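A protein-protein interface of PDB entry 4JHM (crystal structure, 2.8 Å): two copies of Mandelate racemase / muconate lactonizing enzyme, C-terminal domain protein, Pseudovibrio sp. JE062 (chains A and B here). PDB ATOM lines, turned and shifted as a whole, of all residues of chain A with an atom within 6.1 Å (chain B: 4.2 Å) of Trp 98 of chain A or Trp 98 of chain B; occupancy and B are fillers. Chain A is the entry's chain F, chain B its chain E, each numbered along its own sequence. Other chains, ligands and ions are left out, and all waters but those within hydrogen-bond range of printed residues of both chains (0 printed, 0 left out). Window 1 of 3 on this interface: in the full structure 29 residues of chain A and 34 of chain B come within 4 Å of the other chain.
O of Met 55 of chain B is in hydrogen-bond range of NE1 of Trp 98 of chain A, at 3.2 Å.
NE1 of Trp 98 of chain B lies within hydrogen-bond range of O of Met 55 of chain A (3.3 Å).
The side-chain sulfur of Cys 65 of chain A sits at hydrogen-bond distance from the backbone NH of Gly 99 of chain B (3.8 Å).
O of Cys 96 of chain A sits close to O of Tyr 57 of chain B.
O of Trp 98 of chain B sits close to O of Trp 98 of chain A.
OG of Ser 56 of chain A sits at hydrogen-bond distance from ND2 of Asn 38 of chain A, at 2.7 Å.
The side-chain hydroxyl of Ser 56 of chain A lies within hydrogen-bond range of the side-chain carboxylate of Asp 63 of chain A, 3.2 Å away.
The side-chain hydroxyl (OH) of Tyr 57 of chain A is in hydrogen-bond range of the side-chain amide oxygen (OD1) of Asn 249 of chain A (3.4 Å).
The backbone NH (N) of Cys 65 of chain A sits close to the side-chain carboxylate (OD1) of Asp 63 of chain A (3.0 Å).
Among the printed residues, pairs that only touch across the chains: Ser 56 of chain A with Trp 98 of chain B (3.8 Å), Tyr 57 of chain A with Trp 98 of chain B (3.4 Å), Ile 66 of chain A with Trp 98 of chain B (3.7 Å), Trp 98 of chain A with Ser 56 of chain B (3.8 Å), Trp 98 of chain A with Tyr 57 of chain B (3.9 Å), Trp 98 of chain A with Ile 66 of chain B (3.7 Å), Trp 98 of chain A with Pro 102 of chain B (3.4 Å), Trp 98 of chain A with Val 275 of chain B (3.8 Å), Pro 102 of chain A with Trp 98 of chain B (3.7 Å) and Val 275 of chain A with Trp 98 of chain B (3.9 Å).
Printed residues of chain B within 4 Å of Met 55 of chain A: Trp 98 (3.3 Å).
Of the printed residues of chain B, Cys 65 of chain A touches Gly 99 (3.8 Å).
Of chain B, only Met 55, Ser 56, Tyr 57, Ile 66, Trp 98, Pro 102 and Val 275 come within 4 Å of Trp 98 of chain A.
Gly 99 of chain A touches none of the printed residues of chain B.
Asn 249 of chain A touches none of the printed residues of chain B.
The nearest printed residue of chain B that does not touch Trp 98 of chain A is Gly 99 of chain B (4.6 Å).
The nearest printed residue of chain B that does not touch Met 55 of chain A is Thr 97 of chain B (8.6 Å).
Hydrophobic or aromatic side chains of chain A that line the printed part of chain B: Tyr 57, Ile 66, Trp 98, Pro 102 and Val 275.
Among the printed residues, 15 pairs touch across the chains.
Met 55 of chain A touches Trp 98 of chain B, and with the chains exchanged Trp 98 of chain A touches Met 55 of chain B.
Tyr 57 of chain A touches Trp 98 of chain B, and with the chains exchanged Trp 98 of chain A touches Tyr 57 of chain B.
Ile 66 of chain A touches Trp 98 of chain B, and with the chains exchanged Trp 98 of chain A touches Ile 66 of chain B.
Trp 98 of chain A touches Pro 102 of chain B, and with the chains exchanged Pro 102 of chain A touches Trp 98 of chain B.
Positions printed for both chains: 55, 56, 57, 66, 97, 98, 99, 100, 102 and 275.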
ATOM      1  N   ASN A  38      33.564 -31.731   0.136  1.00  0.00           N
ATOM      2  CA  ASN A  38      34.494 -31.794   1.260  1.00  0.00           C
ATOM      3  C   ASN A  38      34.648 -33.229   1.760  1.00  0.00           C
ATOM      4  O   ASN A  38      33.699 -33.811   2.285  1.00  0.00           O
ATOM      5  CB  ASN A  38      34.013 -30.884   2.393  1.00  0.00           C
ATOM      6  CG  ASN A  38      33.892 -29.430   1.963  1.00  0.00           C
ATOM      7  OD1 ASN A  38      34.894 -28.737   1.764  1.00  0.00           O
ATOM      8  ND2 ASN A  38      32.659 -28.959   1.821  1.00  0.00           N
ATOM      9  N   THR A  54      30.651 -34.503   2.706  1.00  0.00           N
ATOM     10  CA  THR A  54      29.504 -33.603   2.781  1.00  0.00           C
ATOM     11  C   THR A  54      29.771 -32.437   1.823  1.00  0.00           C
ATOM     12  O   THR A  54      30.888 -31.916   1.763  1.00  0.00           O
ATOM     13  CB  THR A  54      29.277 -33.066   4.210  1.00  0.00           C
ATOM     14  OG1 THR A  54      28.054 -32.321   4.256  1.00  0.00           O
ATOM     15  CG2 THR A  54      30.430 -32.171   4.651  1.00  0.00           C
ATOM     16  N   MET A  55      28.755 -32.032   1.069  1.00  0.00           N
ATOM     17  CA  MET A  55      28.963 -31.058  -0.001  1.00  0.00           C
ATOM     18  C   MET A  55      28.680 -29.645   0.438  1.00  0.00           C
ATOM     19  O   MET A  55      28.165 -29.408   1.532  1.00  0.00           O
ATOM     20  CB  MET A  55      28.117 -31.471  -1.198  1.00  0.00           C
ATOM     21  CG  MET A  55      26.886 -30.601  -1.382  1.00  0.00           C
ATOM     22  SD  MET A  55      25.910 -31.251  -2.962  1.00  0.00           S
ATOM     23  CE  MET A  55      24.115 -30.842  -2.262  1.00  0.00           C
ATOM     24  N   SER A  56      29.041 -28.694  -0.415  1.00  0.00           N
ATOM     25  CA  SER A  56      28.829 -27.283  -0.135  1.00  0.00           C
ATOM     26  C   SER A  56      28.399 -26.551  -1.395  1.00  0.00           C
ATOM     27  O   SER A  56      28.770 -26.925  -2.506  1.00  0.00           O
ATOM     28  CB  SER A  56      30.108 -26.647   0.403  1.00  0.00           C
ATOM     29  OG  SER A  56      30.554 -27.309   1.568  1.00  0.00           O
ATOM     30  N   TYR A  57      27.614 -25.500  -1.209  1.00  0.00           N
ATOM     31  CA  TYR A  57      27.155 -24.672  -2.308  1.00  0.00           C
ATOM     32  C   TYR A  57      27.361 -23.209  -1.944  1.00  0.00           C
ATOM     33  O   TYR A  57      26.848 -22.725  -0.934  1.00  0.00           O
ATOM     34  CB  TYR A  57      25.685 -24.961  -2.629  1.00  0.00           C
ATOM     35  CG  TYR A  57      24.914 -25.579  -1.486  1.00  0.00           C
ATOM     36  CD1 TYR A  57      24.921 -26.955  -1.283  1.00  0.00           C
ATOM     37  CD2 TYR A  57      24.175 -24.789  -0.606  1.00  0.00           C
ATOM     38  CE1 TYR A  57      24.218 -27.528  -0.235  1.00  0.00           C
ATOM     39  CE2 TYR A  57      23.464 -25.352   0.443  1.00  0.00           C
ATOM     40  CZ  TYR A  57      23.491 -26.721   0.624  1.00  0.00           C
ATOM     41  OH  TYR A  57      22.793 -27.289   1.663  1.00  0.00           O
ATOM     42  N   ASP A  63      34.031 -23.413  -1.801  1.00  0.00           N
ATOM     43  CA  ASP A  63      33.965 -23.256  -0.361  1.00  0.00           C
ATOM     44  C   ASP A  63      35.159 -23.890   0.338  1.00  0.00           C
ATOM     45  O   ASP A  63      35.528 -25.022   0.035  1.00  0.00           O
ATOM     46  CB  ASP A  63      32.675 -23.900   0.151  1.00  0.00           C
ATOM     47  CG  ASP A  63      32.429 -23.630   1.615  1.00  0.00           C
ATOM     48  OD1 ASP A  63      32.719 -22.503   2.065  1.00  0.00           O
ATOM     49  OD2 ASP A  63      31.940 -24.545   2.314  1.00  0.00           O
ATOM     50  N   CYS A  65      35.091 -23.147   3.810  1.00  0.00           N
ATOM     51  CA  CYS A  65      34.498 -23.046   5.136  1.00  0.00           C
ATOM     52  C   CYS A  65      34.517 -24.386   5.876  1.00  0.00           C
ATOM     53  O   CYS A  65      34.898 -24.453   7.043  1.00  0.00           O
ATOM     54  CB  CYS A  65      33.062 -22.540   5.016  1.00  0.00           C
ATOM     55  SG  CYS A  65      32.247 -22.213   6.589  1.00  0.00           S
ATOM     56  N   ILE A  66      34.108 -25.447   5.187  1.00  0.00           N
ATOM     57  CA  ILE A  66      34.020 -26.778   5.787  1.00  0.00           C
ATOM     58  C   ILE A  66      35.393 -27.403   6.034  1.00  0.00           C
ATOM     59  O   ILE A  66      35.640 -27.961   7.099  1.00  0.00           O
ATOM     60  CB  ILE A  66      33.187 -27.728   4.900  1.00  0.00           C
ATOM     61  CG1 ILE A  66      31.720 -27.300   4.897  1.00  0.00           C
ATOM     62  CG2 ILE A  66      33.303 -29.164   5.380  1.00  0.00           C
ATOM     63  CD1 ILE A  66      31.090 -27.277   6.275  1.00  0.00           C
ATOM     64  N   SER A  69      36.861 -25.671   9.018  1.00  0.00           N
ATOM     65  CA  SER A  69      36.199 -26.184  10.213  1.00  0.00           C
ATOM     66  C   SER A  69      36.786 -27.543  10.581  1.00  0.00           C
ATOM     67  O   SER A  69      37.195 -27.765  11.718  1.00  0.00           O
ATOM     68  CB  SER A  69      34.695 -26.323   9.972  1.00  0.00           C
ATOM     69  OG  SER A  69      34.120 -27.273  10.853  1.00  0.00           O
ATOM     70  N   CYS A  96      34.155 -27.409  19.366  1.00  0.00           N
ATOM     71  CA  CYS A  96      33.690 -26.064  19.015  1.00  0.00           C
ATOM     72  C   CYS A  96      34.053 -25.638  17.591  1.00  0.00           C
ATOM     73  O   CYS A  96      35.219 -25.381  17.292  1.00  0.00           O
ATOM     74  CB  CYS A  96      34.285 -25.037  19.979  1.00  0.00           C
ATOM     75  SG  CYS A  96      33.597 -25.060  21.646  1.00  0.00           S
ATOM     76  N   THR A  97      33.049 -25.554  16.724  1.00  0.00           N
ATOM     77  CA  THR A  97      33.210 -24.939  15.408  1.00  0.00           C
ATOM     78  C   THR A  97      31.880 -24.355  14.964  1.00  0.00           C
ATOM     79  O   THR A  97      30.827 -24.933  15.215  1.00  0.00           O
ATOM     80  CB  THR A  97      33.639 -25.946  14.318  1.00  0.00           C
ATOM     81  OG1 THR A  97      34.224 -27.107  14.918  1.00  0.00           O
ATOM     82  CG2 THR A  97      34.629 -25.299  13.340  1.00  0.00           C
ATOM     83  N   TRP A  98      31.936 -23.218  14.288  1.00  0.00           N
ATOM     84  CA  TRP A  98      30.762 -22.662  13.638  1.00  0.00           C
ATOM     85  C   TRP A  98      30.373 -23.484  12.405  1.00  0.00           C
ATOM     86  O   TRP A  98      29.330 -23.241  11.794  1.00  0.00           O
ATOM     87  CB  TRP A  98      31.028 -21.213  13.244  1.00  0.00           C
ATOM     88  CG  TRP A  98      31.201 -20.316  14.419  1.00  0.00           C
ATOM     89  CD1 TRP A  98      32.355 -19.716  14.833  1.00  0.00           C
ATOM     90  CD2 TRP A  98      30.187 -19.923  15.348  1.00  0.00           C
ATOM     91  NE1 TRP A  98      32.119 -18.963  15.959  1.00  0.00           N
ATOM     92  CE2 TRP A  98      30.795 -19.073  16.295  1.00  0.00           C
ATOM     93  CE3 TRP A  98      28.821 -20.203  15.467  1.00  0.00           C
ATOM     94  CZ2 TRP A  98      30.086 -18.499  17.347  1.00  0.00           C
ATOM     95  CZ3 TRP A  98      28.116 -19.633  16.513  1.00  0.00           C
ATOM     96  CH2 TRP A  98      28.750 -18.791  17.440  1.00  0.00           C
ATOM     97  N   GLY A  99      31.221 -24.446  12.042  1.00  0.00           N
ATOM     98  CA  GLY A  99      30.917 -25.397  10.977  1.00  0.00           C
ATOM     99  C   GLY A  99      29.833 -26.388  11.373  1.00  0.00           C
ATOM    100  O   GLY A  99      29.117 -26.909  10.515  1.00  0.00           O
ATOM    101  N   GLY A 100      29.724 -26.665  12.671  1.00  0.00           N
ATOM    102  CA  GLY A 100      28.623 -27.466  13.212  1.00  0.00           C
ATOM    103  C   GLY A 100      28.542 -28.920  12.767  1.00  0.00           C
ATOM    104  O   GLY A 100      29.541 -29.527  12.371  1.00  0.00           O
ATOM    105  N   PRO A 102      27.209 -30.290  10.099  1.00  0.00           N
ATOM    106  CA  PRO A 102      27.577 -30.565   8.710  1.00  0.00           C
ATOM    107  C   PRO A 102      29.066 -30.835   8.539  1.00  0.00           C
ATOM    108  O   PRO A 102      29.449 -31.648   7.701  1.00  0.00           O
ATOM    109  CB  PRO A 102      27.186 -29.278   7.980  1.00  0.00           C
ATOM    110  CG  PRO A 102      26.105 -28.685   8.818  1.00  0.00           C
ATOM    111  CD  PRO A 102      26.481 -29.016  10.232  1.00  0.00           C
ATOM    112  N   ASN A 249      17.599 -29.086   6.277  1.00  0.00           N
ATOM    113  CA  ASN A 249      18.929 -28.565   6.592  1.00  0.00           C
ATOM    114  C   ASN A 249      18.939 -27.524   7.702  1.00  0.00           C
ATOM    115  O   ASN A 249      19.888 -26.747   7.819  1.00  0.00           O
ATOM    116  CB  ASN A 249      19.545 -27.950   5.340  1.00  0.00           C
ATOM    117  CG  ASN A 249      19.936 -28.989   4.319  1.00  0.00           C
ATOM    118  OD1 ASN A 249      20.016 -28.694   3.132  1.00  0.00           O
ATOM    119  ND2 ASN A 249      20.195 -30.211   4.774  1.00  0.00           N
ATOM    120  N   LEU A 252      18.080 -30.047  12.887  1.00  0.00           N
ATOM    121  CA  LEU A 252      18.934 -31.225  12.700  1.00  0.00           C
ATOM    122  C   LEU A 252      18.987 -32.176  13.892  1.00  0.00           C
ATOM    123  O   LEU A 252      19.267 -33.369  13.726  1.00  0.00           O
ATOM    124  CB  LEU A 252      20.364 -30.783  12.374  1.00  0.00           C
ATOM    125  CG  LEU A 252      20.539 -29.864  11.167  1.00  0.00           C
ATOM    126  CD1 LEU A 252      21.991 -29.428  11.039  1.00  0.00           C
ATOM    127  CD2 LEU A 252      20.059 -30.552   9.897  1.00  0.00           C
ATOM    128  N   THR A 274      24.897 -36.311   5.919  1.00  0.00           N
ATOM    129  CA  THR A 274      26.094 -35.490   5.824  1.00  0.00           C
ATOM    130  C   THR A 274      25.880 -34.087   6.384  1.00  0.00           C
ATOM    131  O   THR A 274      26.738 -33.216   6.231  1.00  0.00           O
ATOM    132  CB  THR A 274      26.572 -35.391   4.363  1.00  0.00           C
ATOM    133  OG1 THR A 274      25.599 -34.694   3.574  1.00  0.00           O
ATOM    134  CG2 THR A 274      26.784 -36.779   3.785  1.00  0.00           C
ATOM    135  N   VAL A 275      24.740 -33.875   7.040  1.00  0.00           N
ATOM    136  CA  VAL A 275      24.407 -32.570   7.618  1.00  0.00           C
ATOM    137  C   VAL A 275      24.044 -32.644   9.102  1.00  0.00           C
ATOM    138  O   VAL A 275      24.446 -31.782   9.892  1.00  0.00           O
ATOM    139  CB  VAL A 275      23.230 -31.915   6.867  1.00  0.00           C
ATOM    140  CG1 VAL A 275      22.725 -30.699   7.630  1.00  0.00           C
ATOM    141  CG2 VAL A 275      23.646 -31.534   5.453  1.00  0.00           C
ATOM    142  N   MET B  55      33.480 -13.396  16.695  1.00  0.00           N
ATOM    143  CA  MET B  55      34.633 -14.181  17.153  1.00  0.00           C
ATOM    144  C   MET B  55      34.455 -15.665  16.961  1.00  0.00           C
ATOM    145  O   MET B  55      33.367 -16.139  16.642  1.00  0.00           O
ATOM    146  CB  MET B  55      34.943 -13.859  18.615  1.00  0.00           C
ATOM    147  CG  MET B  55      33.985 -14.531  19.591  1.00  0.00           C
ATOM    148  SD  MET B  55      34.762 -14.460  21.401  1.00  0.00           S
ATOM    149  CE  MET B  55      33.811 -16.017  22.146  1.00  0.00           C
ATOM    150  N   SER B  56      35.548 -16.400  17.138  1.00  0.00           N
ATOM    151  CA  SER B  56      35.555 -17.851  17.003  1.00  0.00           C
ATOM    152  C   SER B  56      36.314 -18.458  18.168  1.00  0.00           C
ATOM    153  O   SER B  56      37.311 -17.900  18.625  1.00  0.00           O
ATOM    154  CB  SER B  56      36.243 -18.277  15.702  1.00  0.00           C
ATOM    155  OG  SER B  56      35.647 -17.680  14.565  1.00  0.00           O
ATOM    156  N   TYR B  57      35.841 -19.598  18.651  1.00  0.00           N
ATOM    157  CA  TYR B  57      36.587 -20.369  19.639  1.00  0.00           C
ATOM    158  C   TYR B  57      36.833 -21.768  19.087  1.00  0.00           C
ATOM    159  O   TYR B  57      35.895 -22.500  18.774  1.00  0.00           O
ATOM    160  CB  TYR B  57      35.858 -20.416  20.990  1.00  0.00           C
ATOM    161  CG  TYR B  57      34.344 -20.446  20.910  1.00  0.00           C
ATOM    162  CD1 TYR B  57      33.608 -19.267  20.861  1.00  0.00           C
ATOM    163  CD2 TYR B  57      33.649 -21.652  20.904  1.00  0.00           C
ATOM    164  CE1 TYR B  57      32.225 -19.287  20.795  1.00  0.00           C
ATOM    165  CE2 TYR B  57      32.265 -21.681  20.839  1.00  0.00           C
ATOM    166  CZ  TYR B  57      31.558 -20.496  20.785  1.00  0.00           C
ATOM    167  OH  TYR B  57      30.183 -20.516  20.724  1.00  0.00           O
ATOM    168  N   ILE B  66      35.348 -18.990   9.589  1.00  0.00           N
ATOM    169  CA  ILE B  66      34.448 -17.848   9.434  1.00  0.00           C
ATOM    170  C   ILE B  66      34.884 -16.873   8.338  1.00  0.00           C
ATOM    171  O   ILE B  66      34.076 -16.482   7.496  1.00  0.00           O
ATOM    172  CB  ILE B  66      34.298 -17.074  10.753  1.00  0.00           C
ATOM    173  CG1 ILE B  66      33.521 -17.908  11.769  1.00  0.00           C
ATOM    174  CG2 ILE B  66      33.590 -15.748  10.520  1.00  0.00           C
ATOM    175  CD1 ILE B  66      32.108 -18.234  11.339  1.00  0.00           C
ATOM    176  N   THR B  97      26.026 -20.397   2.938  1.00  0.00           N
ATOM    177  CA  THR B  97      27.258 -20.789   3.613  1.00  0.00           C
ATOM    178  C   THR B  97      26.893 -21.599   4.832  1.00  0.00           C
ATOM    179  O   THR B  97      25.943 -21.269   5.537  1.00  0.00           O
ATOM    180  CB  THR B  97      28.073 -19.583   4.121  1.00  0.00           C
ATOM    181  OG1 THR B  97      27.696 -18.398   3.413  1.00  0.00           O
ATOM    182  CG2 THR B  97      29.575 -19.839   3.957  1.00  0.00           C
ATOM    183  N   TRP B  98      27.655 -22.652   5.096  1.00  0.00           N
ATOM    184  CA  TRP B  98      27.500 -23.387   6.342  1.00  0.00           C
ATOM    185  C   TRP B  98      27.971 -22.526   7.520  1.00  0.00           C
ATOM    186  O   TRP B  98      27.766 -22.882   8.685  1.00  0.00           O
ATOM    187  CB  TRP B  98      28.261 -24.706   6.283  1.00  0.00           C
ATOM    188  CG  TRP B  98      27.608 -25.721   5.396  1.00  0.00           C
ATOM    189  CD1 TRP B  98      28.157 -26.332   4.309  1.00  0.00           C
ATOM    190  CD2 TRP B  98      26.276 -26.238   5.516  1.00  0.00           C
ATOM    191  NE1 TRP B  98      27.255 -27.201   3.748  1.00  0.00           N
ATOM    192  CE2 TRP B  98      26.091 -27.162   4.469  1.00  0.00           C
ATOM    193  CE3 TRP B  98      25.221 -26.009   6.411  1.00  0.00           C
ATOM    194  CZ2 TRP B  98      24.896 -27.861   4.290  1.00  0.00           C
ATOM    195  CZ3 TRP B  98      24.034 -26.706   6.230  1.00  0.00           C
ATOM    196  CH2 TRP B  98      23.885 -27.620   5.177  1.00  0.00           C
ATOM    197  N   GLY B  99      28.590 -21.389   7.201  1.00  0.00           N
ATOM    198  CA  GLY B  99      28.970 -20.391   8.200  1.00  0.00           C
ATOM    199  C   GLY B  99      27.765 -19.808   8.920  1.00  0.00           C
ATOM    200  O   GLY B  99      27.888 -19.287  10.027  1.00  0.00           O
ATOM    201  N   GLY B 100      26.600 -19.888   8.287  1.00  0.00           N
ATOM    202  CA  GLY B 100      25.348 -19.513   8.934  1.00  0.00           C
ATOM    203  C   GLY B 100      25.276 -18.049   9.324  1.00  0.00           C
ATOM    204  O   GLY B 100      26.000 -17.211   8.776  1.00  0.00           O
ATOM    205  N   PRO B 102      26.110 -16.464  12.142  1.00  0.00           N
ATOM    206  CA  PRO B 102      27.272 -15.861  12.789  1.00  0.00           C
ATOM    207  C   PRO B 102      28.227 -15.253  11.775  1.00  0.00           C
ATOM    208  O   PRO B 102      28.829 -14.214  12.036  1.00  0.00           O
ATOM    209  CB  PRO B 102      27.934 -17.046  13.496  1.00  0.00           C
ATOM    210  CG  PRO B 102      26.832 -18.019  13.720  1.00  0.00           C
ATOM    211  CD  PRO B 102      25.922 -17.869  12.536  1.00  0.00           C
ATOM    212  N   VAL B 275      26.000 -13.024  16.215  1.00  0.00           N
ATOM    213  CA  VAL B 275      25.677 -14.428  15.991  1.00  0.00           C
ATOM    214  C   VAL B 275      24.292 -14.632  15.372  1.00  0.00           C
ATOM    215  O   VAL B 275      24.116 -15.490  14.503  1.00  0.00           O
ATOM    216  CB  VAL B 275      25.740 -15.213  17.307  1.00  0.00           C
ATOM    217  CG1 VAL B 275      25.116 -16.589  17.142  1.00  0.00           C
ATOM    218  CG2 VAL B 275      27.175 -15.311  17.789  1.00  0.00           C
